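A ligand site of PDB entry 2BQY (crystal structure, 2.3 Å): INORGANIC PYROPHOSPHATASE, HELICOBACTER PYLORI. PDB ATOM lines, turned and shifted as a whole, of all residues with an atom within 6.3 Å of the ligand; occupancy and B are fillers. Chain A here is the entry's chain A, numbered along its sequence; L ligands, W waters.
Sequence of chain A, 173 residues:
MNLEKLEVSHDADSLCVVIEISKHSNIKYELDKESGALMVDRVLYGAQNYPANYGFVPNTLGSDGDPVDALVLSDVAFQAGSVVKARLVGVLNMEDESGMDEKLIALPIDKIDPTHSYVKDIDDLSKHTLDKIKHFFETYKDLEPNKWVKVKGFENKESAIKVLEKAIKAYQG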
ATOM      1  N   ILE A  21       8.618   1.928 -26.780  1.00  0.00           N
ATOM      2  CA  ILE A  21       7.250   1.919 -26.305  1.00  0.00           C
ATOM      3  C   ILE A  21       6.742   3.341 -26.178  1.00  0.00           C
ATOM      4  O   ILE A  21       7.421   4.206 -25.648  1.00  0.00           O
ATOM      5  CB  ILE A  21       7.162   1.247 -24.923  1.00  0.00           C
ATOM      6  CG1 ILE A  21       7.878  -0.104 -24.963  1.00  0.00           C
ATOM      7  CG2 ILE A  21       5.713   1.030 -24.564  1.00  0.00           C
ATOM      8  CD1 ILE A  21       8.106  -0.731 -23.566  1.00  0.00           C
ATOM      9  N   LYS A  28       4.427  -3.660 -25.597  1.00  0.00           N
ATOM     10  CA  LYS A  28       5.853  -3.480 -25.379  1.00  0.00           C
ATOM     11  C   LYS A  28       6.707  -3.976 -26.559  1.00  0.00           C
ATOM     12  O   LYS A  28       6.777  -5.185 -26.813  1.00  0.00           O
ATOM     13  CB  LYS A  28       6.271  -4.210 -24.098  1.00  0.00           C
ATOM     14  CG  LYS A  28       7.773  -4.387 -23.929  1.00  0.00           C
ATOM     15  CD  LYS A  28       8.112  -4.904 -22.534  1.00  0.00           C
ATOM     16  CE  LYS A  28       9.598  -5.274 -22.425  1.00  0.00           C
ATOM     17  NZ  LYS A  28      10.503  -4.138 -22.733  1.00  0.00           N
ATOM     18  N   GLU A  30      10.530  -4.041 -28.699  1.00  0.00           N
ATOM     19  CA  GLU A  30      11.949  -4.168 -28.395  1.00  0.00           C
ATOM     20  C   GLU A  30      12.712  -4.188 -29.713  1.00  0.00           C
ATOM     21  O   GLU A  30      12.409  -4.967 -30.600  1.00  0.00           O
ATOM     22  CB  GLU A  30      12.202  -5.459 -27.613  1.00  0.00           C
ATOM     23  CG  GLU A  30      13.624  -5.588 -27.123  1.00  0.00           C
ATOM     24  CD  GLU A  30      13.862  -6.894 -26.389  1.00  0.00           C
ATOM     25  OE1 GLU A  30      13.763  -7.964 -27.058  1.00  0.00           O
ATOM     26  OE2 GLU A  30      14.159  -6.847 -25.160  1.00  0.00           O
ATOM     27  N   ASP A  41       7.619  -7.590 -28.270  1.00  0.00           N
ATOM     28  CA  ASP A  41       8.023  -8.386 -27.101  1.00  0.00           C
ATOM     29  C   ASP A  41       6.839  -8.927 -26.318  1.00  0.00           C
ATOM     30  O   ASP A  41       6.855 -10.091 -25.919  1.00  0.00           O
ATOM     31  CB  ASP A  41       8.922  -7.542 -26.197  1.00  0.00           C
ATOM     32  CG  ASP A  41       9.825  -8.394 -25.324  1.00  0.00           C
ATOM     33  OD1 ASP A  41      10.568  -9.231 -25.869  1.00  0.00           O
ATOM     34  OD2 ASP A  41       9.776  -8.249 -24.093  1.00  0.00           O
ATOM     35  N   ARG A  42       5.828  -8.091 -26.089  1.00  0.00           N
ATOM     36  CA  ARG A  42       4.628  -8.559 -25.391  1.00  0.00           C
ATOM     37  C   ARG A  42       3.525  -7.529 -25.241  1.00  0.00           C
ATOM     38  O   ARG A  42       3.751  -6.343 -25.422  1.00  0.00           O
ATOM     39  CB  ARG A  42       4.978  -9.070 -24.002  1.00  0.00           C
ATOM     40  CG  ARG A  42       5.142  -7.977 -22.977  1.00  0.00           C
ATOM     41  CD  ARG A  42       5.425  -8.547 -21.597  1.00  0.00           C
ATOM     42  NE  ARG A  42       6.432  -9.610 -21.635  1.00  0.00           N
ATOM     43  CZ  ARG A  42       6.138 -10.889 -21.870  1.00  0.00           C
ATOM     44  NH1 ARG A  42       7.097 -11.817 -21.904  1.00  0.00           N
ATOM     45  NH2 ARG A  42       4.864 -11.237 -22.018  1.00  0.00           N
ATOM     46  N   TYR A  50       1.697   1.985 -20.315  1.00  0.00           N
ATOM     47  CA  TYR A  50       2.876   2.722 -19.879  1.00  0.00           C
ATOM     48  C   TYR A  50       2.627   4.164 -19.520  1.00  0.00           C
ATOM     49  O   TYR A  50       1.996   4.880 -20.281  1.00  0.00           O
ATOM     50  CB  TYR A  50       3.987   2.615 -20.924  1.00  0.00           C
ATOM     51  CG  TYR A  50       4.657   1.249 -20.931  1.00  0.00           C
ATOM     52  CD1 TYR A  50       3.988   0.128 -21.419  1.00  0.00           C
ATOM     53  CD2 TYR A  50       5.941   1.086 -20.396  1.00  0.00           C
ATOM     54  CE1 TYR A  50       4.569  -1.129 -21.391  1.00  0.00           C
ATOM     55  CE2 TYR A  50       6.527  -0.172 -20.359  1.00  0.00           C
ATOM     56  CZ  TYR A  50       5.835  -1.278 -20.858  1.00  0.00           C
ATOM     57  OH  TYR A  50       6.409  -2.520 -20.806  1.00  0.00           O
ATOM     58  N   TYR A  54       8.847   4.743 -23.326  1.00  0.00           N
ATOM     59  CA  TYR A  54       9.910   3.859 -22.880  1.00  0.00           C
ATOM     60  C   TYR A  54      10.907   3.567 -24.006  1.00  0.00           C
ATOM     61  O   TYR A  54      10.525   3.275 -25.137  1.00  0.00           O
ATOM     62  CB  TYR A  54       9.318   2.536 -22.387  1.00  0.00           C
ATOM     63  CG  TYR A  54      10.327   1.653 -21.684  1.00  0.00           C
ATOM     64  CD1 TYR A  54      10.578   1.794 -20.317  1.00  0.00           C
ATOM     65  CD2 TYR A  54      11.051   0.672 -22.379  1.00  0.00           C
ATOM     66  CE1 TYR A  54      11.518   1.000 -19.675  1.00  0.00           C
ATOM     67  CE2 TYR A  54      11.990  -0.113 -21.747  1.00  0.00           C
ATOM     68  CZ  TYR A  54      12.214   0.052 -20.402  1.00  0.00           C
ATOM     69  OH  TYR A  54      13.126  -0.726 -19.759  1.00  0.00           O
ATOM     70  N   ASP A  64      21.820  -5.532 -16.901  1.00  0.00           N
ATOM     71  CA  ASP A  64      21.318  -6.800 -17.426  1.00  0.00           C
ATOM     72  C   ASP A  64      21.930  -7.243 -18.749  1.00  0.00           C
ATOM     73  O   ASP A  64      21.450  -8.201 -19.379  1.00  0.00           O
ATOM     74  CB  ASP A  64      19.797  -6.746 -17.557  1.00  0.00           C
ATOM     75  CG  ASP A  64      19.320  -5.750 -18.615  1.00  0.00           C
ATOM     76  OD1 ASP A  64      20.141  -4.934 -19.099  1.00  0.00           O
ATOM     77  OD2 ASP A  64      18.098  -5.793 -18.925  1.00  0.00           O
ATOM     78  N   ASP A  66      21.973  -5.515 -21.506  1.00  0.00           N
ATOM     79  CA  ASP A  66      21.382  -4.759 -22.608  1.00  0.00           C
ATOM     80  C   ASP A  66      21.605  -3.276 -22.362  1.00  0.00           C
ATOM     81  O   ASP A  66      21.911  -2.876 -21.245  1.00  0.00           O
ATOM     82  CB  ASP A  66      19.861  -5.036 -22.721  1.00  0.00           C
ATOM     83  CG  ASP A  66      19.558  -6.470 -23.098  1.00  0.00           C
ATOM     84  OD1 ASP A  66      20.208  -7.004 -24.026  1.00  0.00           O
ATOM     85  OD2 ASP A  66      18.656  -7.058 -22.467  1.00  0.00           O
ATOM     86  N   ASP A  69      18.177   1.248 -19.876  1.00  0.00           N
ATOM     87  CA  ASP A  69      16.840   1.707 -20.193  1.00  0.00           C
ATOM     88  C   ASP A  69      16.575   3.116 -19.670  1.00  0.00           C
ATOM     89  O   ASP A  69      17.215   3.582 -18.713  1.00  0.00           O
ATOM     90  CB  ASP A  69      15.804   0.751 -19.589  1.00  0.00           C
ATOM     91  CG  ASP A  69      15.856  -0.625 -20.202  1.00  0.00           C
ATOM     92  OD1 ASP A  69      15.653  -0.725 -21.439  1.00  0.00           O
ATOM     93  OD2 ASP A  69      16.094  -1.603 -19.431  1.00  0.00           O
ATOM     94  N   MET A  94      14.874  -0.532  -9.024  1.00  0.00           N
ATOM     95  CA  MET A  94      13.949  -1.609  -8.698  1.00  0.00           C
ATOM     96  C   MET A  94      14.648  -2.966  -8.797  1.00  0.00           C
ATOM     97  O   MET A  94      15.779  -3.056  -9.255  1.00  0.00           O
ATOM     98  CB  MET A  94      12.743  -1.582  -9.649  1.00  0.00           C
ATOM     99  CG  MET A  94      13.111  -1.704 -11.119  1.00  0.00           C
ATOM    100  SD  MET A  94      11.676  -1.449 -12.197  1.00  0.00           S
ATOM    101  CE  MET A  94      11.575   0.298 -12.190  1.00  0.00           C
ATOM    102  N   ASP A  96      13.916  -7.134 -10.007  1.00  0.00           N
ATOM    103  CA  ASP A  96      13.030  -8.121 -10.611  1.00  0.00           C
ATOM    104  C   ASP A  96      13.647  -9.516 -10.614  1.00  0.00           C
ATOM    105  O   ASP A  96      14.743  -9.735 -10.109  1.00  0.00           O
ATOM    106  CB  ASP A  96      12.665  -7.707 -12.043  1.00  0.00           C
ATOM    107  CG  ASP A  96      13.878  -7.630 -12.958  1.00  0.00           C
ATOM    108  OD1 ASP A  96      14.880  -8.310 -12.682  1.00  0.00           O
ATOM    109  OD2 ASP A  96      13.795  -6.902 -13.976  1.00  0.00           O
ATOM    110  N   GLU A  97      12.918 -10.472 -11.193  1.00  0.00           N
ATOM    111  CA  GLU A  97      13.366 -11.858 -11.250  1.00  0.00           C
ATOM    112  C   GLU A  97      14.774 -12.010 -11.834  1.00  0.00           C
ATOM    113  O   GLU A  97      15.451 -12.977 -11.535  1.00  0.00           O
ATOM    114  CB  GLU A  97      12.365 -12.708 -12.073  1.00  0.00           C
ATOM    115  CG  GLU A  97      12.369 -12.477 -13.602  1.00  0.00           C
ATOM    116  CD  GLU A  97      11.843 -11.115 -14.004  1.00  0.00           C
ATOM    117  OE1 GLU A  97      10.973 -10.585 -13.283  1.00  0.00           O
ATOM    118  OE2 GLU A  97      12.267 -10.589 -15.049  1.00  0.00           O
ATOM    119  N   SER A  98      15.191 -11.065 -12.667  1.00  0.00           N
ATOM    120  CA  SER A  98      16.512 -11.142 -13.292  1.00  0.00           C
ATOM    121  C   SER A  98      17.602 -10.542 -12.409  1.00  0.00           C
ATOM    122  O   SER A  98      18.752 -10.955 -12.461  1.00  0.00           O
ATOM    123  CB  SER A  98      16.474 -10.425 -14.629  1.00  0.00           C
ATOM    124  OG  SER A  98      17.755 -10.424 -15.218  1.00  0.00           O
ATOM    125  N   ASP A 101      17.481  -3.771 -11.383  1.00  0.00           N
ATOM    126  CA  ASP A 101      17.193  -3.066 -12.636  1.00  0.00           C
ATOM    127  C   ASP A 101      17.221  -1.544 -12.422  1.00  0.00           C
ATOM    128  O   ASP A 101      16.710  -1.012 -11.438  1.00  0.00           O
ATOM    129  CB  ASP A 101      15.825  -3.496 -13.166  1.00  0.00           C
ATOM    130  CG  ASP A 101      15.578  -3.023 -14.579  1.00  0.00           C
ATOM    131  OD1 ASP A 101      14.419  -3.144 -15.025  1.00  0.00           O
ATOM    132  OD2 ASP A 101      16.539  -2.546 -15.232  1.00  0.00           O
ATOM    133  N   LYS A 103      16.357   2.212 -14.223  1.00  0.00           N
ATOM    134  CA  LYS A 103      15.661   2.891 -15.305  1.00  0.00           C
ATOM    135  C   LYS A 103      15.793   4.403 -15.206  1.00  0.00           C
ATOM    136  O   LYS A 103      15.237   5.044 -14.317  1.00  0.00           O
ATOM    137  CB  LYS A 103      14.180   2.487 -15.320  1.00  0.00           C
ATOM    138  CG  LYS A 103      13.996   0.991 -15.395  1.00  0.00           C
ATOM    139  CD  LYS A 103      12.639   0.611 -15.856  1.00  0.00           C
ATOM    140  CE  LYS A 103      12.560  -0.902 -16.090  1.00  0.00           C
ATOM    141  NZ  LYS A 103      13.679  -1.404 -16.929  1.00  0.00           N
ATOM    142  N   PHE A 137       5.252  -0.124 -12.468  1.00  0.00           N
ATOM    143  CA  PHE A 137       6.324  -1.116 -12.485  1.00  0.00           C
ATOM    144  C   PHE A 137       6.172  -2.150 -11.384  1.00  0.00           C
ATOM    145  O   PHE A 137       6.526  -3.336 -11.552  1.00  0.00           O
ATOM    146  CB  PHE A 137       7.667  -0.414 -12.366  1.00  0.00           C
ATOM    147  CG  PHE A 137       8.135   0.220 -13.637  1.00  0.00           C
ATOM    148  CD1 PHE A 137       8.565  -0.558 -14.714  1.00  0.00           C
ATOM    149  CD2 PHE A 137       8.133   1.613 -13.756  1.00  0.00           C
ATOM    150  CE1 PHE A 137       8.984   0.037 -15.915  1.00  0.00           C
ATOM    151  CE2 PHE A 137       8.547   2.211 -14.945  1.00  0.00           C
ATOM    152  CZ  PHE A 137       8.975   1.423 -16.020  1.00  0.00           C
ATOM    153  N   TYR A 140       2.816  -4.142 -13.065  1.00  0.00           N
ATOM    154  CA  TYR A 140       2.632  -4.511 -14.463  1.00  0.00           C
ATOM    155  C   TYR A 140       3.093  -5.928 -14.822  1.00  0.00           C
ATOM    156  O   TYR A 140       2.888  -6.375 -15.962  1.00  0.00           O
ATOM    157  CB  TYR A 140       3.291  -3.471 -15.402  1.00  0.00           C
ATOM    158  CG  TYR A 140       4.770  -3.659 -15.654  1.00  0.00           C
ATOM    159  CD1 TYR A 140       5.674  -3.810 -14.609  1.00  0.00           C
ATOM    160  CD2 TYR A 140       5.264  -3.648 -16.958  1.00  0.00           C
ATOM    161  CE1 TYR A 140       7.038  -3.958 -14.842  1.00  0.00           C
ATOM    162  CE2 TYR A 140       6.630  -3.790 -17.214  1.00  0.00           C
ATOM    163  CZ  TYR A 140       7.519  -3.945 -16.151  1.00  0.00           C
ATOM    164  OH  TYR A 140       8.874  -4.075 -16.414  1.00  0.00           O
ATOM    165  N   LYS A 141       3.714  -6.621 -13.870  1.00  0.00           N
ATOM    166  CA  LYS A 141       4.171  -7.989 -14.120  1.00  0.00           C
ATOM    167  C   LYS A 141       3.566  -8.982 -13.142  1.00  0.00           C
ATOM    168  O   LYS A 141       4.018 -10.109 -13.060  1.00  0.00           O
ATOM    169  CB  LYS A 141       5.703  -8.081 -14.092  1.00  0.00           C
ATOM    170  CG  LYS A 141       6.366  -7.652 -15.399  1.00  0.00           C
ATOM    171  CD  LYS A 141       7.745  -8.261 -15.569  1.00  0.00           C
ATOM    172  CE  LYS A 141       8.831  -7.474 -14.893  1.00  0.00           C
ATOM    173  NZ  LYS A 141      10.176  -8.172 -14.954  1.00  0.00           N
ATOM    174  N   GLU A 144       2.183 -12.152 -14.865  1.00  0.00           N
ATOM    175  CA  GLU A 144       3.131 -12.891 -15.677  1.00  0.00           C
ATOM    176  C   GLU A 144       3.877 -13.920 -14.832  1.00  0.00           C
ATOM    177  O   GLU A 144       4.680 -13.572 -13.988  1.00  0.00           O
ATOM    178  CB  GLU A 144       4.142 -11.938 -16.335  1.00  0.00           C
ATOM    179  CG  GLU A 144       3.542 -11.097 -17.437  1.00  0.00           C
ATOM    180  CD  GLU A 144       4.582 -10.276 -18.168  1.00  0.00           C
ATOM    181  OE1 GLU A 144       5.617 -10.869 -18.532  1.00  0.00           O
ATOM    182  OE2 GLU A 144       4.348  -9.068 -18.401  1.00  0.00           O
ATOM    183  N   LYS A 147       7.480 -14.038 -12.820  1.00  0.00           N
ATOM    184  CA  LYS A 147       8.017 -12.701 -13.044  1.00  0.00           C
ATOM    185  C   LYS A 147       7.505 -11.785 -11.937  1.00  0.00           C
ATOM    186  O   LYS A 147       6.362 -11.959 -11.459  1.00  0.00           O
ATOM    187  CB  LYS A 147       7.572 -12.156 -14.413  1.00  0.00           C
ATOM    188  CG  LYS A 147       8.217 -12.854 -15.595  1.00  0.00           C
ATOM    189  CD  LYS A 147       7.760 -12.223 -16.897  1.00  0.00           C
ATOM    190  CE  LYS A 147       8.305 -12.986 -18.105  1.00  0.00           C
ATOM    191  NZ  LYS A 147       9.801 -13.158 -17.978  1.00  0.00           N
ATOM    192  N   VAL A 149       8.452  -7.675  -9.686  1.00  0.00           N
ATOM    193  CA  VAL A 149       9.204  -6.438  -9.519  1.00  0.00           C
ATOM    194  C   VAL A 149       9.014  -5.908  -8.099  1.00  0.00           C
ATOM    195  O   VAL A 149       7.924  -5.987  -7.540  1.00  0.00           O
ATOM    196  CB  VAL A 149       8.722  -5.349 -10.524  1.00  0.00           C
ATOM    197  CG1 VAL A 149       9.470  -4.047 -10.282  1.00  0.00           C
ATOM    198  CG2 VAL A 149       8.951  -5.825 -11.943  1.00  0.00           C
HETATM  199  P1  LIG L   1      11.537  -6.795 -18.363  1.00  0.00           P
HETATM  200  O1  LIG L   1      10.339  -7.663 -18.805  1.00  0.00           O
HETATM  201  O2  LIG L   1      12.972  -7.339 -18.829  1.00  0.00           O
HETATM  202  O3  LIG L   1      11.525  -6.535 -16.824  1.00  0.00           O
HETATM  203  O4  LIG L   1      11.293  -5.341 -19.158  1.00  0.00           O
HETATM  204  P2  LIG L   1      12.361  -4.063 -18.998  1.00  0.00           P
HETATM  205  O5  LIG L   1      13.749  -4.538 -19.489  1.00  0.00           O
HETATM  206  O6  LIG L   1      11.751  -2.986 -19.876  1.00  0.00           O
HETATM  207  O7  LIG L   1      12.382  -3.681 -17.492  1.00  0.00           O
HETATM  208  O   HOH W   1       8.226  -7.354 -20.564  1.00  0.00           O
HETATM  209  O   HOH W   2      16.591  -4.059 -21.365  1.00  0.00           O
HETATM  210  O   HOH W   3      11.815  -4.624 -14.400  1.00  0.00           O
HETATM  211  O   HOH W   4      14.439  -8.942 -16.211  1.00  0.00           O
HETATM  212  O   HOH W   5       9.068  -2.650 -19.744  1.00  0.00           O
HETATM  213  O   HOH W   6      16.277  -7.981 -18.440  1.00  0.00           O
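O7 of the ligand lies close to OD1 of Asp 101, 3.2 Å away. OD2 of Asp 69 touches O5 of the ligand, at 3.8 Å. Asp 96 touches the ligand (OD2 to O3, 3.7 Å). Tyr 140 touches the ligand. The nearest printed residue that does not touch the ligand is Glu 97 (4.5 Å).
Water W5 lies within hydrogen-bond range of O6 of the ligand and OH of Tyr 50. Water W1 bridges an oxygen (O1) of the ligand (2.8 Å) and the guanidinium group (NE) of Arg 42 (3.1 Å). Water W3 lies within hydrogen-bond range of OD2 of Asp 96, OD1 of Asp 101 and O3 of the ligand. Water W6 lies within hydrogen-bond range of OD2 of Asp 64 and O2 of the ligand. Water W4 lies within hydrogen-bond range of the side-chain carboxylate (OE2) of Glu 97 (3.0 Å), the side-chain carboxylate (OD2) of Asp 96 (3.1 Å) and an oxygen (O2) of the ligand (3.4 Å). Water W2 lies within hydrogen-bond range of OD2 of Asp 69 (3.2 Å), OD2 of Asp 64 (3.4 Å) and O5 of the ligand (3.4 Å).
The side-chain hydroxyl of Tyr 54 sits close to the side-chain carboxylate of Asp 69 (3.0 Å). The backbone carbonyl oxygen (O) of Ile 21 sits at hydrogen-bond distance from the backbone NH (N) of Tyr 54 (2.8 Å). The side-chain carboxylate (OD1) of Asp 101 lies within salt-bridge range of the side-chain amino group (NZ) of Lys 103 (2.7 Å). The side-chain amino group (NZ) of Lys 103 is in salt-bridge range of the side-chain carboxylate (OD2) of Asp 69, at 3.5 Å. The side-chain amino group (NZ) of Lys 141 is in salt-bridge range of the side-chain carboxylate (OD2) of Asp 96, at 3.96 Å. The side-chain amino group (NZ) of Lys 141 lies within salt-bridge range of the side-chain carboxylate (OE1) of Glu 97, 3.0 Å away. The backbone NH (N) of Asp 101 is in hydrogen-bond range of the backbone carbonyl oxygen (O) of Met 94. The side-chain carboxylate (OD1) of Asp 96 lies within hydrogen-bond range of the backbone NH (N) of Ser 98, at 2.8 Å.
The side-chain hydroxyl (OH) of Tyr 54 is in hydrogen-bond range of an oxygen (O6) of the ligand, at 2.6 Å. O7 of the ligand is in salt-bridge range of NZ of Lys 103. The side-chain amino group (NZ) of Lys 141 lies within salt-bridge range of an oxygen (O3) of the ligand (2.8 Å). NZ of Lys 28 lies within salt-bridge range of O6 of the ligand, at 3.3 Å.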
